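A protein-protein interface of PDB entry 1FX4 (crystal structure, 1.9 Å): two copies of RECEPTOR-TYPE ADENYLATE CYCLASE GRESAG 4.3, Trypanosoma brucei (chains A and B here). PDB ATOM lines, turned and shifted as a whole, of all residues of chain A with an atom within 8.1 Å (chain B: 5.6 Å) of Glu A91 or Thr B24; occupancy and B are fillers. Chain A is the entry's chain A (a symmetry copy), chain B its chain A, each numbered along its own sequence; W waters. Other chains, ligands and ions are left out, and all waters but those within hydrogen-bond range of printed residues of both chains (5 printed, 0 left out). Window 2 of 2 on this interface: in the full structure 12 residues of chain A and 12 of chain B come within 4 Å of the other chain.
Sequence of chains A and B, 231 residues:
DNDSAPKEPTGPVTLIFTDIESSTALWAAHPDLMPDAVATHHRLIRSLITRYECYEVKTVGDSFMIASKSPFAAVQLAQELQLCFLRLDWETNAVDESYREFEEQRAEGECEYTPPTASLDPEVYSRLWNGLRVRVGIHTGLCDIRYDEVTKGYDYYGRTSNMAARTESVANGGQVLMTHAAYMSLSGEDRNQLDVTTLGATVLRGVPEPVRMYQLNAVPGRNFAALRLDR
OG1 of Thr B24 lies within hydrogen-bond range of OE2 of Glu A91 (3.3 Å). The guanidinium group (NH2) of Arg B228 is in salt-bridge range of the side-chain carboxylate (OD2) of Asp A89 (3.5 Å).
Among the printed residues, pairs that only touch across the chains: Asp A36 with Thr B24, Asp A36 with Ala B28 and Arg A43 with Trp B27.
Water W2 lies within hydrogen-bond range of OG1 of Thr A40 (2.6 Å) and OG1 of Thr B24 (2.9 Å). Water W4 lies within hydrogen-bond range of the backbone carbonyl oxygen of Thr B24 (2.6 Å) and the side-chain carboxylate of Asp A36 (2.7 Å). Water W1 lies within hydrogen-bond range of the backbone carbonyl oxygen (O) of Asp A89 (2.7 Å), the side-chain hydroxyl (OG1) of Thr B24 (3.0 Å) and the side-chain carboxylate (OE2) of Glu A91 (3.4 Å). Water W3 bridges the side-chain carboxylate of Glu A91 and the backbone NH of Ala B25. Water W5 lies within hydrogen-bond range of NH1 of Arg B228 (3.0 Å) and OE1 of Glu A91 (3.1 Å).
Of the printed residues of chain B, Asp A36 touches Thr B24 (3.2 Å) and Ala B28 (3.6 Å). Of the printed residues of chain B, Arg A43 touches Trp B27 (3.4 Å). Printed residues of chain B within 4 Å of Asp A89: Arg B228 (3.5 Å). Glu A91 touches just one residue of chain B: Thr B24. No residue of chain A comes within 4 Å of Ser B23. Of chain A, only Asp A36 and Glu A91 come within 4 Å of Thr B24. No residue of chain A comes within 4 Å of Ala B25. Of the printed residues of chain A, Ala B28 touches Asp A36 (3.6 Å). The nearest residue of chain B that does not touch Glu A91 is Ser B23 (4.4 Å). The nearest residue of chain A that does not touch Thr B24 is Thr A40 (4.2 Å).
O of Asp A36 lies within hydrogen-bond range of OG1 of Thr A40. The guanidinium group of Arg A43 is in hydrogen-bond range of the side-chain hydroxyl of Thr A40. The side-chain carboxylate (OD1) of Asp A89 sits at hydrogen-bond distance from the backbone NH (N) of Glu A91.
Printed residues of chain B that touch a printed residue of chain A: Thr B24, Trp B27, Ala B28 and Arg B228. Hydrophobic or aromatic side chains of chain B within 4 Å of the printed part of chain A: Trp B27 and Ala B28.
No position is printed for both chains.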
ATOM      1  N   ASP A  32     -31.335  15.975 -10.927  1.00  0.00           N
ATOM      2  CA  ASP A  32     -31.401  17.226 -10.180  1.00  0.00           C
ATOM      3  C   ASP A  32     -30.097  17.603  -9.478  1.00  0.00           C
ATOM      4  O   ASP A  32     -29.931  18.738  -9.055  1.00  0.00           O
ATOM      5  CB  ASP A  32     -32.529  17.146  -9.143  1.00  0.00           C
ATOM      6  CG  ASP A  32     -32.361  15.975  -8.164  1.00  0.00           C
ATOM      7  OD1 ASP A  32     -32.164  14.817  -8.608  1.00  0.00           O
ATOM      8  OD2 ASP A  32     -32.436  16.221  -6.935  1.00  0.00           O
ATOM      9  N   LEU A  33     -29.194  16.641  -9.320  1.00  0.00           N
ATOM     10  CA  LEU A  33     -27.922  16.907  -8.653  1.00  0.00           C
ATOM     11  C   LEU A  33     -26.736  16.918  -9.592  1.00  0.00           C
ATOM     12  O   LEU A  33     -25.776  17.658  -9.377  1.00  0.00           O
ATOM     13  CB  LEU A  33     -27.645  15.849  -7.586  1.00  0.00           C
ATOM     14  CG  LEU A  33     -28.655  15.712  -6.454  1.00  0.00           C
ATOM     15  CD1 LEU A  33     -28.239  14.554  -5.581  1.00  0.00           C
ATOM     16  CD2 LEU A  33     -28.721  16.999  -5.645  1.00  0.00           C
ATOM     17  N   PRO A  35     -26.137  18.037 -12.849  1.00  0.00           N
ATOM     18  CA  PRO A  35     -25.645  19.203 -13.594  1.00  0.00           C
ATOM     19  C   PRO A  35     -24.684  20.043 -12.757  1.00  0.00           C
ATOM     20  O   PRO A  35     -23.609  20.424 -13.232  1.00  0.00           O
ATOM     21  CB  PRO A  35     -26.928  19.973 -13.917  1.00  0.00           C
ATOM     22  CG  PRO A  35     -27.935  18.871 -14.086  1.00  0.00           C
ATOM     23  CD  PRO A  35     -27.608  17.960 -12.916  1.00  0.00           C
ATOM     24  N   ASP A  36     -25.061  20.283 -11.505  1.00  0.00           N
ATOM     25  CA  ASP A  36     -24.236  21.076 -10.591  1.00  0.00           C
ATOM     26  C   ASP A  36     -22.971  20.346 -10.156  1.00  0.00           C
ATOM     27  O   ASP A  36     -21.900  20.937 -10.077  1.00  0.00           O
ATOM     28  CB  ASP A  36     -25.033  21.444  -9.344  1.00  0.00           C
ATOM     29  CG  ASP A  36     -26.161  22.418  -9.631  1.00  0.00           C
ATOM     30  OD1 ASP A  36     -26.125  23.120 -10.671  1.00  0.00           O
ATOM     31  OD2 ASP A  36     -27.091  22.484  -8.797  1.00  0.00           O
ATOM     32  N   ALA A  37     -23.109  19.065  -9.839  1.00  0.00           N
ATOM     33  CA  ALA A  37     -21.972  18.261  -9.391  1.00  0.00           C
ATOM     34  C   ALA A  37     -20.923  18.168 -10.492  1.00  0.00           C
ATOM     35  O   ALA A  37     -19.739  18.339 -10.230  1.00  0.00           O
ATOM     36  CB  ALA A  37     -22.426  16.871  -8.959  1.00  0.00           C
ATOM     37  N   VAL A  38     -21.363  17.951 -11.730  1.00  0.00           N
ATOM     38  CA  VAL A  38     -20.433  17.862 -12.846  1.00  0.00           C
ATOM     39  C   VAL A  38     -19.811  19.219 -13.150  1.00  0.00           C
ATOM     40  O   VAL A  38     -18.645  19.293 -13.513  1.00  0.00           O
ATOM     41  CB  VAL A  38     -21.090  17.281 -14.114  1.00  0.00           C
ATOM     42  CG1 VAL A  38     -20.112  17.351 -15.284  1.00  0.00           C
ATOM     43  CG2 VAL A  38     -21.488  15.836 -13.859  1.00  0.00           C
ATOM     44  N   ALA A  39     -20.588  20.286 -12.992  1.00  0.00           N
ATOM     45  CA  ALA A  39     -20.071  21.627 -13.234  1.00  0.00           C
ATOM     46  C   ALA A  39     -18.972  21.897 -12.201  1.00  0.00           C
ATOM     47  O   ALA A  39     -17.946  22.478 -12.525  1.00  0.00           O
ATOM     48  CB  ALA A  39     -21.190  22.662 -13.111  1.00  0.00           C
ATOM     49  N   THR A  40     -19.191  21.446 -10.967  1.00  0.00           N
ATOM     50  CA  THR A  40     -18.209  21.623  -9.893  1.00  0.00           C
ATOM     51  C   THR A  40     -16.959  20.814 -10.253  1.00  0.00           C
ATOM     52  O   THR A  40     -15.833  21.303 -10.151  1.00  0.00           O
ATOM     53  CB  THR A  40     -18.798  21.158  -8.541  1.00  0.00           C
ATOM     54  OG1 THR A  40     -19.921  21.990  -8.215  1.00  0.00           O
ATOM     55  CG2 THR A  40     -17.772  21.245  -7.427  1.00  0.00           C
ATOM     56  N   ARG A  43     -14.913  22.625 -12.758  1.00  0.00           N
ATOM     57  CA  ARG A  43     -14.222  23.773 -12.166  1.00  0.00           C
ATOM     58  C   ARG A  43     -13.020  23.330 -11.339  1.00  0.00           C
ATOM     59  O   ARG A  43     -11.959  23.938 -11.412  1.00  0.00           O
ATOM     60  CB  ARG A  43     -15.165  24.599 -11.287  1.00  0.00           C
ATOM     61  CG  ARG A  43     -16.001  25.596 -12.024  1.00  0.00           C
ATOM     62  CD  ARG A  43     -16.576  26.635 -11.054  1.00  0.00           C
ATOM     63  NE  ARG A  43     -17.064  26.026  -9.817  1.00  0.00           N
ATOM     64  CZ  ARG A  43     -18.250  25.433  -9.674  1.00  0.00           C
ATOM     65  NH1 ARG A  43     -19.101  25.369 -10.689  1.00  0.00           N
ATOM     66  NH2 ARG A  43     -18.564  24.876  -8.511  1.00  0.00           N
ATOM     67  N   LEU A  88     -14.144  18.427  -0.758  1.00  0.00           N
ATOM     68  CA  LEU A  88     -15.232  19.330  -1.110  1.00  0.00           C
ATOM     69  C   LEU A  88     -16.580  18.948  -0.500  1.00  0.00           C
ATOM     70  O   LEU A  88     -16.895  17.766  -0.391  1.00  0.00           O
ATOM     71  CB  LEU A  88     -15.401  19.380  -2.626  1.00  0.00           C
ATOM     72  CG  LEU A  88     -16.368  20.493  -3.032  1.00  0.00           C
ATOM     73  CD1 LEU A  88     -15.609  21.569  -3.792  1.00  0.00           C
ATOM     74  CD2 LEU A  88     -17.515  19.944  -3.863  1.00  0.00           C
ATOM     75  N   ASP A  89     -17.359  19.946  -0.077  1.00  0.00           N
ATOM     76  CA  ASP A  89     -18.693  19.686   0.441  1.00  0.00           C
ATOM     77  C   ASP A  89     -19.585  19.725  -0.791  1.00  0.00           C
ATOM     78  O   ASP A  89     -19.829  20.796  -1.352  1.00  0.00           O
ATOM     79  CB  ASP A  89     -19.141  20.753   1.447  1.00  0.00           C
ATOM     80  CG  ASP A  89     -20.618  20.611   1.849  1.00  0.00           C
ATOM     81  OD1 ASP A  89     -21.266  19.583   1.520  1.00  0.00           O
ATOM     82  OD2 ASP A  89     -21.137  21.536   2.513  1.00  0.00           O
ATOM     83  N   TRP A  90     -20.050  18.550  -1.208  1.00  0.00           N
ATOM     84  CA  TRP A  90     -20.901  18.405  -2.379  1.00  0.00           C
ATOM     85  C   TRP A  90     -22.347  18.799  -2.120  1.00  0.00           C
ATOM     86  O   TRP A  90     -23.159  18.863  -3.055  1.00  0.00           O
ATOM     87  CB  TRP A  90     -20.825  16.968  -2.893  1.00  0.00           C
ATOM     88  CG  TRP A  90     -19.468  16.631  -3.411  1.00  0.00           C
ATOM     89  CD1 TRP A  90     -18.417  16.148  -2.694  1.00  0.00           C
ATOM     90  CD2 TRP A  90     -19.003  16.794  -4.754  1.00  0.00           C
ATOM     91  NE1 TRP A  90     -17.322  16.001  -3.502  1.00  0.00           N
ATOM     92  CE2 TRP A  90     -17.653  16.391  -4.771  1.00  0.00           C
ATOM     93  CE3 TRP A  90     -19.597  17.248  -5.941  1.00  0.00           C
ATOM     94  CZ2 TRP A  90     -16.877  16.427  -5.939  1.00  0.00           C
ATOM     95  CZ3 TRP A  90     -18.832  17.286  -7.096  1.00  0.00           C
ATOM     96  CH2 TRP A  90     -17.481  16.878  -7.087  1.00  0.00           C
ATOM     97  N   GLU A  91     -22.661  19.054  -0.846  1.00  0.00           N
ATOM     98  CA  GLU A  91     -23.998  19.472  -0.427  1.00  0.00           C
ATOM     99  C   GLU A  91     -25.061  18.415  -0.678  1.00  0.00           C
ATOM    100  O   GLU A  91     -26.222  18.737  -0.917  1.00  0.00           O
ATOM    101  CB  GLU A  91     -24.400  20.787  -1.105  1.00  0.00           C
ATOM    102  CG  GLU A  91     -23.471  21.962  -0.836  1.00  0.00           C
ATOM    103  CD  GLU A  91     -23.886  23.213  -1.603  1.00  0.00           C
ATOM    104  OE1 GLU A  91     -25.110  23.433  -1.760  1.00  0.00           O
ATOM    105  OE2 GLU A  91     -22.997  23.972  -2.065  1.00  0.00           O
ATOM    106  N   THR A  92     -24.654  17.154  -0.633  1.00  0.00           N
ATOM    107  CA  THR A  92     -25.569  16.041  -0.831  1.00  0.00           C
ATOM    108  C   THR A  92     -24.873  14.748  -0.457  1.00  0.00           C
ATOM    109  O   THR A  92     -23.652  14.652  -0.555  1.00  0.00           O
ATOM    110  CB  THR A  92     -26.050  15.943  -2.310  1.00  0.00           C
ATOM    111  OG1 THR A  92     -26.971  14.857  -2.434  1.00  0.00           O
ATOM    112  CG2 THR A  92     -24.868  15.692  -3.266  1.00  0.00           C
ATOM    113  N   ASN A  93     -25.628  13.784   0.057  1.00  0.00           N
ATOM    114  CA  ASN A  93     -25.031  12.506   0.364  1.00  0.00           C
ATOM    115  C   ASN A  93     -25.580  11.508  -0.643  1.00  0.00           C
ATOM    116  O   ASN A  93     -25.190  10.345  -0.644  1.00  0.00           O
ATOM    117  CB  ASN A  93     -25.337  12.050   1.794  1.00  0.00           C
ATOM    118  CG  ASN A  93     -24.319  11.027   2.303  1.00  0.00           C
ATOM    119  OD1 ASN A  93     -23.173  11.378   2.600  1.00  0.00           O
ATOM    120  ND2 ASN A  93     -24.721   9.756   2.368  1.00  0.00           N
ATOM    121  N   ALA A  94     -26.445  11.998  -1.532  1.00  0.00           N
ATOM    122  CA  ALA A  94     -27.086  11.162  -2.544  1.00  0.00           C
ATOM    123  C   ALA A  94     -26.128  10.442  -3.497  1.00  0.00           C
ATOM    124  O   ALA A  94     -26.402   9.315  -3.914  1.00  0.00           O
ATOM    125  CB  ALA A  94     -28.096  11.989  -3.336  1.00  0.00           C
ATOM    126  N   VAL A  95     -25.020  11.090  -3.846  1.00  0.00           N
ATOM    127  CA  VAL A  95     -24.042  10.486  -4.761  1.00  0.00           C
ATOM    128  C   VAL A  95     -23.356   9.295  -4.075  1.00  0.00           C
ATOM    129  O   VAL A  95     -23.164   8.246  -4.677  1.00  0.00           O
ATOM    130  CB  VAL A  95     -23.000  11.533  -5.168  1.00  0.00           C
ATOM    131  CG1 VAL A  95     -21.945  10.987  -6.131  1.00  0.00           C
ATOM    132  CG2 VAL A  95     -23.611  12.750  -5.865  1.00  0.00           C
ATOM    133  N   ASN A 130     -16.277  10.674  -0.631  1.00  0.00           N
ATOM    134  CA  ASN A 130     -17.220  11.770  -0.570  1.00  0.00           C
ATOM    135  C   ASN A 130     -17.406  12.402  -1.949  1.00  0.00           C
ATOM    136  O   ASN A 130     -16.458  12.926  -2.528  1.00  0.00           O
ATOM    137  CB  ASN A 130     -16.719  12.845   0.405  1.00  0.00           C
ATOM    138  CG  ASN A 130     -17.601  14.074   0.423  1.00  0.00           C
ATOM    139  OD1 ASN A 130     -18.828  13.978   0.428  1.00  0.00           O
ATOM    140  ND2 ASN A 130     -16.977  15.242   0.420  1.00  0.00           N
ATOM    141  N   GLY A 131     -18.624  12.332  -2.473  1.00  0.00           N
ATOM    142  CA  GLY A 131     -18.925  12.940  -3.765  1.00  0.00           C
ATOM    143  C   GLY A 131     -18.586  12.133  -5.001  1.00  0.00           C
ATOM    144  O   GLY A 131     -18.475  10.917  -4.949  1.00  0.00           O
ATOM    145  N   ILE B  20     -18.457  29.303   0.774  1.00  0.00           N
ATOM    146  CA  ILE B  20     -19.448  30.228   0.266  1.00  0.00           C
ATOM    147  C   ILE B  20     -20.794  29.526   0.329  1.00  0.00           C
ATOM    148  O   ILE B  20     -20.967  28.434  -0.234  1.00  0.00           O
ATOM    149  CB  ILE B  20     -19.156  30.640  -1.177  1.00  0.00           C
ATOM    150  CG1 ILE B  20     -17.832  31.412  -1.245  1.00  0.00           C
ATOM    151  CG2 ILE B  20     -20.285  31.527  -1.703  1.00  0.00           C
ATOM    152  CD1 ILE B  20     -17.497  31.854  -2.653  1.00  0.00           C
ATOM    153  N   SER B  22     -24.313  28.362  -0.546  1.00  0.00           N
ATOM    154  CA  SER B  22     -25.046  28.189  -1.805  1.00  0.00           C
ATOM    155  C   SER B  22     -24.244  28.499  -3.048  1.00  0.00           C
ATOM    156  O   SER B  22     -24.821  28.915  -4.052  1.00  0.00           O
ATOM    157  CB  SER B  22     -26.278  29.093  -1.818  1.00  0.00           C
ATOM    158  OG  SER B  22     -27.211  28.656  -0.873  1.00  0.00           O
ATOM    159  N   SER B  23     -22.934  28.278  -3.022  1.00  0.00           N
ATOM    160  CA  SER B  23     -22.151  28.599  -4.208  1.00  0.00           C
ATOM    161  C   SER B  23     -22.557  27.770  -5.424  1.00  0.00           C
ATOM    162  O   SER B  23     -22.557  28.263  -6.542  1.00  0.00           O
ATOM    163  CB  SER B  23     -20.650  28.484  -3.952  1.00  0.00           C
ATOM    164  OG  SER B  23     -20.260  27.165  -3.649  1.00  0.00           O
ATOM    165  N   THR B  24     -22.915  26.515  -5.198  1.00  0.00           N
ATOM    166  CA  THR B  24     -23.324  25.660  -6.310  1.00  0.00           C
ATOM    167  C   THR B  24     -24.536  26.264  -7.027  1.00  0.00           C
ATOM    168  O   THR B  24     -24.517  26.454  -8.242  1.00  0.00           O
ATOM    169  CB  THR B  24     -23.611  24.242  -5.809  1.00  0.00           C
ATOM    170  OG1 THR B  24     -22.402  23.697  -5.280  1.00  0.00           O
ATOM    171  CG2 THR B  24     -24.073  23.361  -6.939  1.00  0.00           C
ATOM    172  N   ALA B  25     -25.552  26.640  -6.261  1.00  0.00           N
ATOM    173  CA  ALA B  25     -26.762  27.247  -6.817  1.00  0.00           C
ATOM    174  C   ALA B  25     -26.470  28.608  -7.458  1.00  0.00           C
ATOM    175  O   ALA B  25     -27.106  28.991  -8.436  1.00  0.00           O
ATOM    176  CB  ALA B  25     -27.826  27.379  -5.743  1.00  0.00           C
ATOM    177  N   LEU B  26     -25.509  29.347  -6.898  1.00  0.00           N
ATOM    178  CA  LEU B  26     -25.134  30.637  -7.464  1.00  0.00           C
ATOM    179  C   LEU B  26     -24.422  30.436  -8.799  1.00  0.00           C
ATOM    180  O   LEU B  26     -24.627  31.210  -9.742  1.00  0.00           O
ATOM    181  CB  LEU B  26     -24.232  31.424  -6.492  1.00  0.00           C
ATOM    182  CG  LEU B  26     -24.942  31.912  -5.226  1.00  0.00           C
ATOM    183  CD1 LEU B  26     -23.930  32.648  -4.310  1.00  0.00           C
ATOM    184  CD2 LEU B  26     -26.057  32.857  -5.619  1.00  0.00           C
ATOM    185  N   TRP B  27     -23.574  29.410  -8.880  1.00  0.00           N
ATOM    186  CA  TRP B  27     -22.848  29.122 -10.111  1.00  0.00           C
ATOM    187  C   TRP B  27     -23.838  28.772 -11.215  1.00  0.00           C
ATOM    188  O   TRP B  27     -23.661  29.160 -12.361  1.00  0.00           O
ATOM    189  CB  TRP B  27     -21.874  27.958  -9.928  1.00  0.00           C
ATOM    190  CG  TRP B  27     -20.512  28.380  -9.475  1.00  0.00           C
ATOM    191  CD1 TRP B  27     -19.979  28.221  -8.234  1.00  0.00           C
ATOM    192  CD2 TRP B  27     -19.503  29.017 -10.269  1.00  0.00           C
ATOM    193  NE1 TRP B  27     -18.706  28.716  -8.202  1.00  0.00           N
ATOM    194  CE2 TRP B  27     -18.387  29.206  -9.436  1.00  0.00           C
ATOM    195  CE3 TRP B  27     -19.430  29.428 -11.603  1.00  0.00           C
ATOM    196  CZ2 TRP B  27     -17.204  29.803  -9.894  1.00  0.00           C
ATOM    197  CZ3 TRP B  27     -18.256  30.016 -12.058  1.00  0.00           C
ATOM    198  CH2 TRP B  27     -17.159  30.194 -11.205  1.00  0.00           C
ATOM    199  N   ALA B  28     -24.891  28.056 -10.837  1.00  0.00           N
ATOM    200  CA  ALA B  28     -25.921  27.646 -11.784  1.00  0.00           C
ATOM    201  C   ALA B  28     -26.732  28.849 -12.250  1.00  0.00           C
ATOM    202  O   ALA B  28     -26.978  29.011 -13.438  1.00  0.00           O
ATOM    203  CB  ALA B  28     -26.837  26.608 -11.137  1.00  0.00           C
ATOM    204  N   ALA B  29     -27.100  29.718 -11.311  1.00  0.00           N
ATOM    205  CA  ALA B  29     -27.892  30.891 -11.640  1.00  0.00           C
ATOM    206  C   ALA B  29     -27.103  32.053 -12.253  1.00  0.00           C
ATOM    207  O   ALA B  29     -27.648  32.819 -13.049  1.00  0.00           O
ATOM    208  CB  ALA B  29     -28.640  31.368 -10.404  1.00  0.00           C
ATOM    209  N   ARG B 228     -27.045  24.414  10.594  1.00  0.00           N
ATOM    210  CA  ARG B 228     -27.189  23.355   9.585  1.00  0.00           C
ATOM    211  C   ARG B 228     -26.878  21.964  10.136  1.00  0.00           C
ATOM    212  O   ARG B 228     -25.968  21.298   9.638  1.00  0.00           O
ATOM    213  CB  ARG B 228     -26.241  23.597   8.403  1.00  0.00           C
ATOM    214  CG  ARG B 228     -26.545  24.772   7.502  1.00  0.00           C
ATOM    215  CD  ARG B 228     -25.291  25.181   6.724  1.00  0.00           C
ATOM    216  NE  ARG B 228     -24.602  24.061   6.076  1.00  0.00           N
ATOM    217  CZ  ARG B 228     -24.546  23.877   4.762  1.00  0.00           C
ATOM    218  NH1 ARG B 228     -25.150  24.737   3.948  1.00  0.00           N
ATOM    219  NH2 ARG B 228     -23.848  22.867   4.256  1.00  0.00           N
HETATM  220  O   HOH W   1     -20.540  22.148  -3.594  1.00  0.00           O
HETATM  221  O   HOH W   2     -21.178  21.182  -6.048  1.00  0.00           O
HETATM  222  O   HOH W   3     -26.076  25.468  -3.483  1.00  0.00           O
HETATM  223  O   HOH W   4     -24.006  24.712 -10.171  1.00  0.00           O
HETATM  224  O   HOH W   5     -25.596  23.458   1.327  1.00  0.00           O
